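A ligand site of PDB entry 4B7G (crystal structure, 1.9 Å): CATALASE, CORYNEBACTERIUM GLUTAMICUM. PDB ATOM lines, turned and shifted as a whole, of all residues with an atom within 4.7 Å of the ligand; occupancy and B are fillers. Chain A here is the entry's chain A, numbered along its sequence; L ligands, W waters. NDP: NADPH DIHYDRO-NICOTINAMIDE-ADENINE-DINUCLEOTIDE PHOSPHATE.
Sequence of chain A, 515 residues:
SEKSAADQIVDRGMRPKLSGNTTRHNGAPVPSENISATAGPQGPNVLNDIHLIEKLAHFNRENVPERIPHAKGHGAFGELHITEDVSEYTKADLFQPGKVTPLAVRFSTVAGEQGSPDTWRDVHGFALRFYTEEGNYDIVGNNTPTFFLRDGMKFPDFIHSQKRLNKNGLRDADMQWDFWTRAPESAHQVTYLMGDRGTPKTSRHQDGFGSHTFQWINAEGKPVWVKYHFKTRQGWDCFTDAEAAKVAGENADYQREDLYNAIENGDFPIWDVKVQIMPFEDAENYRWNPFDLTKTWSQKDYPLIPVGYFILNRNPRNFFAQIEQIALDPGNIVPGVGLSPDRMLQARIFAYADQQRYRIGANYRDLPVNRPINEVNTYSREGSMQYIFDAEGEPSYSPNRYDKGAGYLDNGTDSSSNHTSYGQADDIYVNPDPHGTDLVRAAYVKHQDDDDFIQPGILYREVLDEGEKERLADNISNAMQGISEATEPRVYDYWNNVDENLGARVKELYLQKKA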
ATOM      1  N   PRO A 145     -28.676 -30.150   3.338  1.00  0.00           N
ATOM      2  CA  PRO A 145     -28.198 -30.155   1.952  1.00  0.00           C
ATOM      3  C   PRO A 145     -28.326 -31.538   1.313  1.00  0.00           C
ATOM      4  O   PRO A 145     -28.028 -31.673   0.128  1.00  0.00           O
ATOM      5  CB  PRO A 145     -26.699 -29.824   2.120  1.00  0.00           C
ATOM      6  CG  PRO A 145     -26.347 -30.467   3.453  1.00  0.00           C
ATOM      7  CD  PRO A 145     -27.566 -30.131   4.307  1.00  0.00           C
ATOM      8  N   HIS A 188     -25.764 -40.708   5.737  1.00  0.00           N
ATOM      9  CA  HIS A 188     -25.393 -39.291   5.679  1.00  0.00           C
ATOM     10  C   HIS A 188     -26.447 -38.413   6.382  1.00  0.00           C
ATOM     11  O   HIS A 188     -26.126 -37.631   7.279  1.00  0.00           O
ATOM     12  CB  HIS A 188     -25.199 -38.841   4.231  1.00  0.00           C
ATOM     13  CG  HIS A 188     -24.488 -37.524   4.086  1.00  0.00           C
ATOM     14  ND1 HIS A 188     -24.201 -36.962   2.854  1.00  0.00           N
ATOM     15  CD2 HIS A 188     -24.009 -36.656   5.006  1.00  0.00           C
ATOM     16  CE1 HIS A 188     -23.582 -35.808   3.036  1.00  0.00           C
ATOM     17  NE2 HIS A 188     -23.440 -35.607   4.331  1.00  0.00           N
ATOM     18  N   TYR A 192     -26.582 -36.151  10.081  1.00  0.00           N
ATOM     19  CA  TYR A 192     -26.968 -34.740  10.139  1.00  0.00           C
ATOM     20  C   TYR A 192     -28.150 -34.561  11.099  1.00  0.00           C
ATOM     21  O   TYR A 192     -28.174 -33.648  11.935  1.00  0.00           O
ATOM     22  CB  TYR A 192     -27.352 -34.295   8.733  1.00  0.00           C
ATOM     23  CG  TYR A 192     -27.557 -32.820   8.515  1.00  0.00           C
ATOM     24  CD1 TYR A 192     -28.757 -32.203   8.854  1.00  0.00           C
ATOM     25  CD2 TYR A 192     -26.566 -32.044   7.911  1.00  0.00           C
ATOM     26  CE1 TYR A 192     -28.962 -30.849   8.622  1.00  0.00           C
ATOM     27  CE2 TYR A 192     -26.772 -30.689   7.680  1.00  0.00           C
ATOM     28  CZ  TYR A 192     -27.976 -30.108   8.041  1.00  0.00           C
ATOM     29  OH  TYR A 192     -28.182 -28.763   7.808  1.00  0.00           O
ATOM     30  N   ASP A 196     -26.642 -31.574  16.218  1.00  0.00           N
ATOM     31  CA  ASP A 196     -27.293 -30.364  16.701  1.00  0.00           C
ATOM     32  C   ASP A 196     -28.410 -29.880  15.771  1.00  0.00           C
ATOM     33  O   ASP A 196     -29.452 -29.413  16.229  1.00  0.00           O
ATOM     34  CB  ASP A 196     -26.269 -29.230  16.828  1.00  0.00           C
ATOM     35  CG  ASP A 196     -25.284 -29.438  17.953  1.00  0.00           C
ATOM     36  OD1 ASP A 196     -25.269 -30.524  18.588  1.00  0.00           O
ATOM     37  OD2 ASP A 196     -24.501 -28.505  18.200  1.00  0.00           O
ATOM     38  N   ARG A 197     -28.191 -29.994  14.469  1.00  0.00           N
ATOM     39  CA  ARG A 197     -29.134 -29.415  13.514  1.00  0.00           C
ATOM     40  C   ARG A 197     -30.468 -30.174  13.420  1.00  0.00           C
ATOM     41  O   ARG A 197     -31.386 -29.757  12.692  1.00  0.00           O
ATOM     42  CB  ARG A 197     -28.482 -29.263  12.146  1.00  0.00           C
ATOM     43  CG  ARG A 197     -27.284 -28.306  12.173  1.00  0.00           C
ATOM     44  CD  ARG A 197     -26.779 -28.043  10.771  1.00  0.00           C
ATOM     45  NE  ARG A 197     -25.670 -27.084  10.769  1.00  0.00           N
ATOM     46  CZ  ARG A 197     -25.157 -26.584   9.651  1.00  0.00           C
ATOM     47  NH1 ARG A 197     -25.646 -26.944   8.463  1.00  0.00           N
ATOM     48  NH2 ARG A 197     -24.154 -25.723   9.721  1.00  0.00           N
ATOM     49  N   PHE A 209     -31.955 -25.432   1.968  1.00  0.00           N
ATOM     50  CA  PHE A 209     -31.225 -25.977   0.817  1.00  0.00           C
ATOM     51  C   PHE A 209     -32.189 -26.538  -0.214  1.00  0.00           C
ATOM     52  O   PHE A 209     -33.255 -27.051   0.137  1.00  0.00           O
ATOM     53  CB  PHE A 209     -30.322 -27.123   1.264  1.00  0.00           C
ATOM     54  CG  PHE A 209     -29.360 -26.747   2.351  1.00  0.00           C
ATOM     55  CD1 PHE A 209     -29.732 -26.843   3.687  1.00  0.00           C
ATOM     56  CD2 PHE A 209     -28.055 -26.334   2.044  1.00  0.00           C
ATOM     57  CE1 PHE A 209     -28.848 -26.509   4.706  1.00  0.00           C
ATOM     58  CE2 PHE A 209     -27.159 -25.989   3.056  1.00  0.00           C
ATOM     59  CZ  PHE A 209     -27.551 -26.073   4.393  1.00  0.00           C
ATOM     60  N   HIS A 229     -28.312 -22.841  -1.895  1.00  0.00           N
ATOM     61  CA  HIS A 229     -28.037 -22.728  -0.471  1.00  0.00           C
ATOM     62  C   HIS A 229     -28.643 -21.436   0.043  1.00  0.00           C
ATOM     63  O   HIS A 229     -28.365 -20.353  -0.491  1.00  0.00           O
ATOM     64  CB  HIS A 229     -26.521 -22.690  -0.236  1.00  0.00           C
ATOM     65  CG  HIS A 229     -25.843 -24.011  -0.441  1.00  0.00           C
ATOM     66  ND1 HIS A 229     -25.702 -24.581  -1.689  1.00  0.00           N
ATOM     67  CD2 HIS A 229     -25.260 -24.852   0.434  1.00  0.00           C
ATOM     68  CE1 HIS A 229     -25.055 -25.732  -1.566  1.00  0.00           C
ATOM     69  NE2 HIS A 229     -24.777 -25.918  -0.283  1.00  0.00           N
ATOM     70  N   LYS A 231     -28.594 -19.222   3.166  1.00  0.00           N
ATOM     71  CA  LYS A 231     -27.788 -19.116   4.377  1.00  0.00           C
ATOM     72  C   LYS A 231     -28.389 -18.106   5.358  1.00  0.00           C
ATOM     73  O   LYS A 231     -28.511 -16.904   5.043  1.00  0.00           O
ATOM     74  CB  LYS A 231     -26.343 -18.737   4.038  1.00  0.00           C
ATOM     75  CG  LYS A 231     -25.659 -19.652   3.012  1.00  0.00           C
ATOM     76  CD  LYS A 231     -25.515 -21.100   3.516  1.00  0.00           C
ATOM     77  CE  LYS A 231     -24.500 -21.199   4.646  1.00  0.00           C
ATOM     78  NZ  LYS A 231     -24.322 -22.606   5.141  1.00  0.00           N
ATOM     79  N   GLN A 276     -23.995 -23.324  -5.608  1.00  0.00           N
ATOM     80  CA  GLN A 276     -22.804 -23.974  -6.129  1.00  0.00           C
ATOM     81  C   GLN A 276     -23.052 -24.169  -7.608  1.00  0.00           C
ATOM     82  O   GLN A 276     -24.184 -24.458  -8.017  1.00  0.00           O
ATOM     83  CB  GLN A 276     -22.586 -25.329  -5.455  1.00  0.00           C
ATOM     84  CG  GLN A 276     -22.227 -25.245  -3.977  1.00  0.00           C
ATOM     85  CD  GLN A 276     -22.118 -26.623  -3.350  1.00  0.00           C
ATOM     86  OE1 GLN A 276     -23.101 -27.353  -3.268  1.00  0.00           O
ATOM     87  NE2 GLN A 276     -20.898 -26.989  -2.929  1.00  0.00           N
ATOM     88  N   THR A 296     -23.422 -34.694  -0.999  1.00  0.00           N
ATOM     89  CA  THR A 296     -23.202 -33.264  -1.161  1.00  0.00           C
ATOM     90  C   THR A 296     -22.010 -32.980  -2.079  1.00  0.00           C
ATOM     91  O   THR A 296     -21.128 -33.830  -2.261  1.00  0.00           O
ATOM     92  CB  THR A 296     -22.967 -32.562   0.202  1.00  0.00           C
ATOM     93  OG1 THR A 296     -21.898 -33.209   0.900  1.00  0.00           O
ATOM     94  CG2 THR A 296     -24.243 -32.610   1.056  1.00  0.00           C
ATOM     95  N   TRP A 297     -21.989 -31.794  -2.670  1.00  0.00           N
ATOM     96  CA  TRP A 297     -20.798 -31.329  -3.377  1.00  0.00           C
ATOM     97  C   TRP A 297     -19.915 -30.593  -2.370  1.00  0.00           C
ATOM     98  O   TRP A 297     -20.392 -29.688  -1.664  1.00  0.00           O
ATOM     99  CB  TRP A 297     -21.156 -30.335  -4.476  1.00  0.00           C
ATOM    100  CG  TRP A 297     -21.977 -30.863  -5.619  1.00  0.00           C
ATOM    101  CD1 TRP A 297     -22.298 -32.163  -5.901  1.00  0.00           C
ATOM    102  CD2 TRP A 297     -22.571 -30.069  -6.658  1.00  0.00           C
ATOM    103  NE1 TRP A 297     -23.063 -32.212  -7.056  1.00  0.00           N
ATOM    104  CE2 TRP A 297     -23.245 -30.932  -7.526  1.00  0.00           C
ATOM    105  CE3 TRP A 297     -22.600 -28.683  -6.907  1.00  0.00           C
ATOM    106  CZ2 TRP A 297     -23.934 -30.470  -8.652  1.00  0.00           C
ATOM    107  CZ3 TRP A 297     -23.271 -28.227  -8.012  1.00  0.00           C
ATOM    108  CH2 TRP A 297     -23.939 -29.123  -8.874  1.00  0.00           C
ATOM    109  N   SER A 298     -18.647 -30.972  -2.296  1.00  0.00           N
ATOM    110  CA  SER A 298     -17.753 -30.284  -1.359  1.00  0.00           C
ATOM    111  C   SER A 298     -17.644 -28.798  -1.696  1.00  0.00           C
ATOM    112  O   SER A 298     -17.482 -28.434  -2.867  1.00  0.00           O
ATOM    113  CB  SER A 298     -16.361 -30.905  -1.351  1.00  0.00           C
ATOM    114  OG  SER A 298     -15.499 -30.128  -0.533  1.00  0.00           O
ATOM    115  N   GLN A 299     -17.759 -27.944  -0.686  1.00  0.00           N
ATOM    116  CA  GLN A 299     -17.646 -26.508  -0.890  1.00  0.00           C
ATOM    117  C   GLN A 299     -16.188 -26.086  -1.096  1.00  0.00           C
ATOM    118  O   GLN A 299     -15.912 -24.919  -1.388  1.00  0.00           O
ATOM    119  CB  GLN A 299     -18.296 -25.746   0.272  1.00  0.00           C
ATOM    120  CG  GLN A 299     -19.821 -25.938   0.334  1.00  0.00           C
ATOM    121  CD  GLN A 299     -20.423 -25.664   1.700  1.00  0.00           C
ATOM    122  OE1 GLN A 299     -20.212 -26.412   2.659  1.00  0.00           O
ATOM    123  NE2 GLN A 299     -21.187 -24.583   1.808  1.00  0.00           N
ATOM    124  N   LYS A 300     -15.260 -27.035  -0.966  1.00  0.00           N
ATOM    125  CA  LYS A 300     -13.868 -26.777  -1.294  1.00  0.00           C
ATOM    126  C   LYS A 300     -13.703 -26.897  -2.798  1.00  0.00           C
ATOM    127  O   LYS A 300     -12.828 -26.267  -3.391  1.00  0.00           O
ATOM    128  CB  LYS A 300     -12.942 -27.764  -0.587  1.00  0.00           C
ATOM    129  CG  LYS A 300     -13.198 -27.870   0.903  1.00  0.00           C
ATOM    130  CD  LYS A 300     -12.137 -28.730   1.588  1.00  0.00           C
ATOM    131  CE  LYS A 300     -12.588 -29.179   2.979  1.00  0.00           C
ATOM    132  NZ  LYS A 300     -11.484 -29.840   3.729  1.00  0.00           N
ATOM    133  N   GLN A 455     -19.140 -39.714   3.468  1.00  0.00           N
ATOM    134  CA  GLN A 455     -19.474 -38.312   3.745  1.00  0.00           C
ATOM    135  C   GLN A 455     -19.897 -37.994   5.180  1.00  0.00           C
ATOM    136  O   GLN A 455     -19.444 -36.987   5.736  1.00  0.00           O
ATOM    137  CB  GLN A 455     -20.508 -37.785   2.730  1.00  0.00           C
ATOM    138  CG  GLN A 455     -19.920 -37.608   1.319  1.00  0.00           C
ATOM    139  CD  GLN A 455     -20.780 -36.705   0.448  1.00  0.00           C
ATOM    140  OE1 GLN A 455     -21.975 -36.567   0.671  1.00  0.00           O
ATOM    141  NE2 GLN A 455     -20.153 -36.067  -0.538  1.00  0.00           N
ATOM    142  N   ILE A 458     -16.666 -38.084   7.072  1.00  0.00           N
ATOM    143  CA  ILE A 458     -15.908 -36.852   6.874  1.00  0.00           C
ATOM    144  C   ILE A 458     -16.469 -35.728   7.738  1.00  0.00           C
ATOM    145  O   ILE A 458     -15.711 -34.951   8.350  1.00  0.00           O
ATOM    146  CB  ILE A 458     -15.913 -36.400   5.395  1.00  0.00           C
ATOM    147  CG1 ILE A 458     -15.043 -37.334   4.539  1.00  0.00           C
ATOM    148  CG2 ILE A 458     -15.441 -34.952   5.252  1.00  0.00           C
ATOM    149  CD1 ILE A 458     -15.222 -37.150   3.030  1.00  0.00           C
ATOM    150  N   LEU A 459     -17.795 -35.628   7.796  1.00  0.00           N
ATOM    151  CA  LEU A 459     -18.452 -34.663   8.670  1.00  0.00           C
ATOM    152  C   LEU A 459     -17.974 -34.845  10.108  1.00  0.00           C
ATOM    153  O   LEU A 459     -17.608 -33.888  10.788  1.00  0.00           O
ATOM    154  CB  LEU A 459     -19.962 -34.825   8.585  1.00  0.00           C
ATOM    155  CG  LEU A 459     -20.811 -33.998   9.556  1.00  0.00           C
ATOM    156  CD1 LEU A 459     -20.590 -32.512   9.322  1.00  0.00           C
ATOM    157  CD2 LEU A 459     -22.300 -34.374   9.451  1.00  0.00           C
ATOM    158  N   VAL A 463     -15.132 -32.062  10.249  1.00  0.00           N
ATOM    159  CA  VAL A 463     -15.965 -30.864  10.362  1.00  0.00           C
ATOM    160  C   VAL A 463     -16.447 -30.548  11.780  1.00  0.00           C
ATOM    161  O   VAL A 463     -16.300 -29.421  12.267  1.00  0.00           O
ATOM    162  CB  VAL A 463     -17.182 -30.921   9.416  1.00  0.00           C
ATOM    163  CG1 VAL A 463     -18.008 -29.650   9.524  1.00  0.00           C
ATOM    164  CG2 VAL A 463     -16.729 -31.130   7.986  1.00  0.00           C
ATOM    165  N   LEU A 464     -17.030 -31.542  12.444  1.00  0.00           N
ATOM    166  CA  LEU A 464     -17.642 -31.308  13.760  1.00  0.00           C
ATOM    167  C   LEU A 464     -16.598 -30.944  14.822  1.00  0.00           C
ATOM    168  O   LEU A 464     -15.485 -31.464  14.791  1.00  0.00           O
ATOM    169  CB  LEU A 464     -18.395 -32.574  14.219  1.00  0.00           C
ATOM    170  CG  LEU A 464     -19.540 -33.074  13.356  1.00  0.00           C
ATOM    171  CD1 LEU A 464     -20.300 -34.214  14.044  1.00  0.00           C
ATOM    172  CD2 LEU A 464     -20.480 -31.925  13.008  1.00  0.00           C
ATOM    173  N   GLU A 468     -19.842 -31.077  19.475  1.00  0.00           N
ATOM    174  CA  GLU A 468     -20.787 -31.599  18.494  1.00  0.00           C
ATOM    175  C   GLU A 468     -20.677 -33.115  18.356  1.00  0.00           C
ATOM    176  O   GLU A 468     -21.693 -33.807  18.267  1.00  0.00           O
ATOM    177  CB  GLU A 468     -20.569 -30.915  17.147  1.00  0.00           C
ATOM    178  CG  GLU A 468     -21.031 -29.463  17.083  1.00  0.00           C
ATOM    179  CD  GLU A 468     -20.657 -28.791  15.780  1.00  0.00           C
ATOM    180  OE1 GLU A 468     -19.508 -28.988  15.315  1.00  0.00           O
ATOM    181  OE2 GLU A 468     -21.487 -28.046  15.218  1.00  0.00           O
HETATM  182  PA  NDP L   1     -16.782 -27.573   4.449  1.00  0.00           P
HETATM  183  O1A NDP L   1     -16.489 -26.644   3.322  1.00  0.00           O
HETATM  184  O2A NDP L   1     -15.851 -27.380   5.588  1.00  0.00           O
HETATM  185  O5B NDP L   1     -18.277 -27.336   4.999  1.00  0.00           O
HETATM  186  C5B NDP L   1     -18.804 -28.204   5.971  1.00  0.00           C
HETATM  187  C4B NDP L   1     -20.257 -27.811   6.197  1.00  0.00           C
HETATM  188  O4B NDP L   1     -20.789 -28.497   7.328  1.00  0.00           O
HETATM  189  C3B NDP L   1     -20.399 -26.316   6.451  1.00  0.00           C
HETATM  190  O3B NDP L   1     -21.465 -25.832   5.650  1.00  0.00           O
HETATM  191  C2B NDP L   1     -20.748 -26.258   7.924  1.00  0.00           C
HETATM  192  O2B NDP L   1     -21.530 -25.139   8.303  1.00  0.00           O
HETATM  193  C1B NDP L   1     -21.502 -27.559   8.109  1.00  0.00           C
HETATM  194  N9A NDP L   1     -21.675 -27.915   9.537  1.00  0.00           N
HETATM  195  C8A NDP L   1     -21.048 -27.360  10.624  1.00  0.00           C
HETATM  196  N7A NDP L   1     -21.521 -27.964  11.736  1.00  0.00           N
HETATM  197  C5A NDP L   1     -22.445 -28.885  11.385  1.00  0.00           C
HETATM  198  C6A NDP L   1     -23.227 -29.779  12.130  1.00  0.00           C
HETATM  199  N6A NDP L   1     -23.370 -29.591  13.445  1.00  0.00           N
HETATM  200  N1A NDP L   1     -24.099 -30.629  11.471  1.00  0.00           N
HETATM  201  C2A NDP L   1     -24.182 -30.591  10.087  1.00  0.00           C
HETATM  202  N3A NDP L   1     -23.402 -29.701   9.361  1.00  0.00           N
HETATM  203  C4A NDP L   1     -22.559 -28.864   9.994  1.00  0.00           C
HETATM  204  O3  NDP L   1     -16.748 -29.116   3.980  1.00  0.00           O
HETATM  205  PN  NDP L   1     -17.536 -29.741   2.697  1.00  0.00           P
HETATM  206  O1N NDP L   1     -18.360 -28.699   2.032  1.00  0.00           O
HETATM  207  O2N NDP L   1     -16.548 -30.527   1.924  1.00  0.00           O
HETATM  208  O5D NDP L   1     -18.495 -30.844   3.383  1.00  0.00           O
HETATM  209  C5D NDP L   1     -17.993 -31.619   4.458  1.00  0.00           C
HETATM  210  C4D NDP L   1     -19.145 -32.287   5.190  1.00  0.00           C
HETATM  211  O4D NDP L   1     -20.015 -31.299   5.739  1.00  0.00           O
HETATM  212  C3D NDP L   1     -19.992 -33.129   4.238  1.00  0.00           C
HETATM  213  O3D NDP L   1     -19.562 -34.485   4.195  1.00  0.00           O
HETATM  214  C2D NDP L   1     -21.403 -32.969   4.781  1.00  0.00           C
HETATM  215  O2D NDP L   1     -21.726 -34.025   5.643  1.00  0.00           O
HETATM  216  C1D NDP L   1     -21.379 -31.676   5.596  1.00  0.00           C
HETATM  217  N1N NDP L   1     -22.159 -30.606   4.930  1.00  0.00           N
HETATM  218  C2N NDP L   1     -21.965 -30.356   3.606  1.00  0.00           C
HETATM  219  C3N NDP L   1     -22.500 -29.229   2.967  1.00  0.00           C
HETATM  220  C7N NDP L   1     -22.218 -29.030   1.509  1.00  0.00           C
HETATM  221  O7N NDP L   1     -20.974 -29.448   0.989  1.00  0.00           O
HETATM  222  N7N NDP L   1     -23.115 -28.456   0.712  1.00  0.00           N
HETATM  223  C4N NDP L   1     -23.345 -28.226   3.727  1.00  0.00           C
HETATM  224  C5N NDP L   1     -23.512 -28.606   5.171  1.00  0.00           C
HETATM  225  C6N NDP L   1     -22.929 -29.762   5.687  1.00  0.00           C
HETATM  226  P2B NDP L   1     -20.800 -23.832   8.886  1.00  0.00           P
HETATM  227  O1X NDP L   1     -19.961 -24.255  10.066  1.00  0.00           O
HETATM  228  O2X NDP L   1     -19.964 -23.198   7.796  1.00  0.00           O
HETATM  229  O3X NDP L   1     -21.855 -22.854   9.352  1.00  0.00           O
HETATM  230  O   HOH W   1     -24.194 -25.811   6.122  1.00  0.00           O
HETATM  231  O   HOH W   2     -23.538 -32.181  15.175  1.00  0.00           O
HETATM  232  O   HOH W   3     -23.768 -29.588  -1.683  1.00  0.00           O
HETATM  233  O   HOH W   4     -17.963 -34.504   1.916  1.00  0.00           O
HETATM  234  O   HOH W   5     -17.403 -23.745   6.812  1.00  0.00           O
HETATM  235  O   HOH W   6     -26.321 -31.836  12.683  1.00  0.00           O
HETATM  236  O   HOH W   7     -23.816 -22.888   7.935  1.00  0.00           O
HETATM  237  O   HOH W   8     -20.528 -24.885  12.516  1.00  0.00           O
HETATM  238  O   HOH W   9     -17.604 -24.241   3.955  1.00  0.00           O
HETATM  239  O   HOH W  10     -14.001 -29.487   6.268  1.00  0.00           O
HETATM  240  O   HOH W  11     -21.607 -22.943   5.557  1.00  0.00           O
HETATM  241  O   HOH W  12     -15.641 -33.353   1.728  1.00  0.00           O
HETATM  242  O   HOH W  13     -22.972 -21.867  11.526  1.00  0.00           O
HETATM  243  O   HOH W  14     -17.596 -25.741  10.226  1.00  0.00           O
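NE2 of His 188 is in hydrogen-bond range of O2D of the ligand (2.7 Å).
The side-chain hydroxyl (OG) of Ser 298 is in hydrogen-bond range of an oxygen (O2N) of the ligand.
O7N of the ligand lies close to O of Trp 297, 2.7 Å away.
N of Gln 299 sits at hydrogen-bond distance from O1N of the ligand (2.9 Å).
The side-chain amide oxygen (OE1) of Gln 299 sits close to an oxygen (O1N) of the ligand, at 3.0 Å.
O of Gln 455 lies within hydrogen-bond range of O3D of the ligand, at 2.9 Å.
OE2 of Glu 468 is in hydrogen-bond range of N6A of the ligand (3.0 Å).
NH2 of Arg 197 lies within salt-bridge range of O3X of the ligand (3.7 Å).
NE2 of His 229 sits at hydrogen-bond distance from N7N of the ligand, at 3.2 Å.
A ring nitrogen (ND1) of His 188 sits close to the side-chain amide oxygen (OE1) of Gln 455 (3.1 Å).
The side-chain hydroxyl (OG) of Ser 298 lies close to the backbone NH (N) of Lys 300, at 3.1 Å.
O of Trp 297 is in hydrogen-bond range of NE2 of Gln 276 (3.0 Å).
OE1 of Gln 455 sits at hydrogen-bond distance from N of Thr 296 (2.9 Å).
The side-chain hydroxyl (OH) of Tyr 192 is in hydrogen-bond range of the guanidinium group (NH1) of Arg 197 (3.2 Å).
The backbone NH of Leu 464 lies within hydrogen-bond range of the backbone carbonyl oxygen of Leu 459 (2.9 Å).
Merely in contact with the ligand: Leu 459, Tyr 192, Leu 464, Val 463, Pro 145 and Thr 296.
Hydrophobic or aromatic side chains within 4 Å of the ligand: Pro 145, His 188, Tyr 192, Leu 459, Val 463 and Leu 464.
Water W7 lies within hydrogen-bond range of O3X of the ligand (2.4 Å), NZ of Lys 231 (2.9 Å) and NH2 of Arg 197 (3.4 Å).
Water W3 lies within hydrogen-bond range of N7N of the ligand (2.7 Å), OE1 of Gln 276 (2.8 Å) and N of Trp 297 (3.0 Å).
Water W1 lies within hydrogen-bond range of O3B of the ligand (2.8 Å), NH1 of Arg 197 (3.0 Å) and NZ of Lys 231 (3.4 Å).
Water W11 bridges the side-chain amino group of Lys 231 and an oxygen (O2X) of the ligand.
Water W6 lies within hydrogen-bond range of O of Tyr 192, N1A of the ligand and N of Arg 197.
Water W2 lies within hydrogen-bond range of a nitrogen (N6A) of the ligand and the backbone NH of Asp 196.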
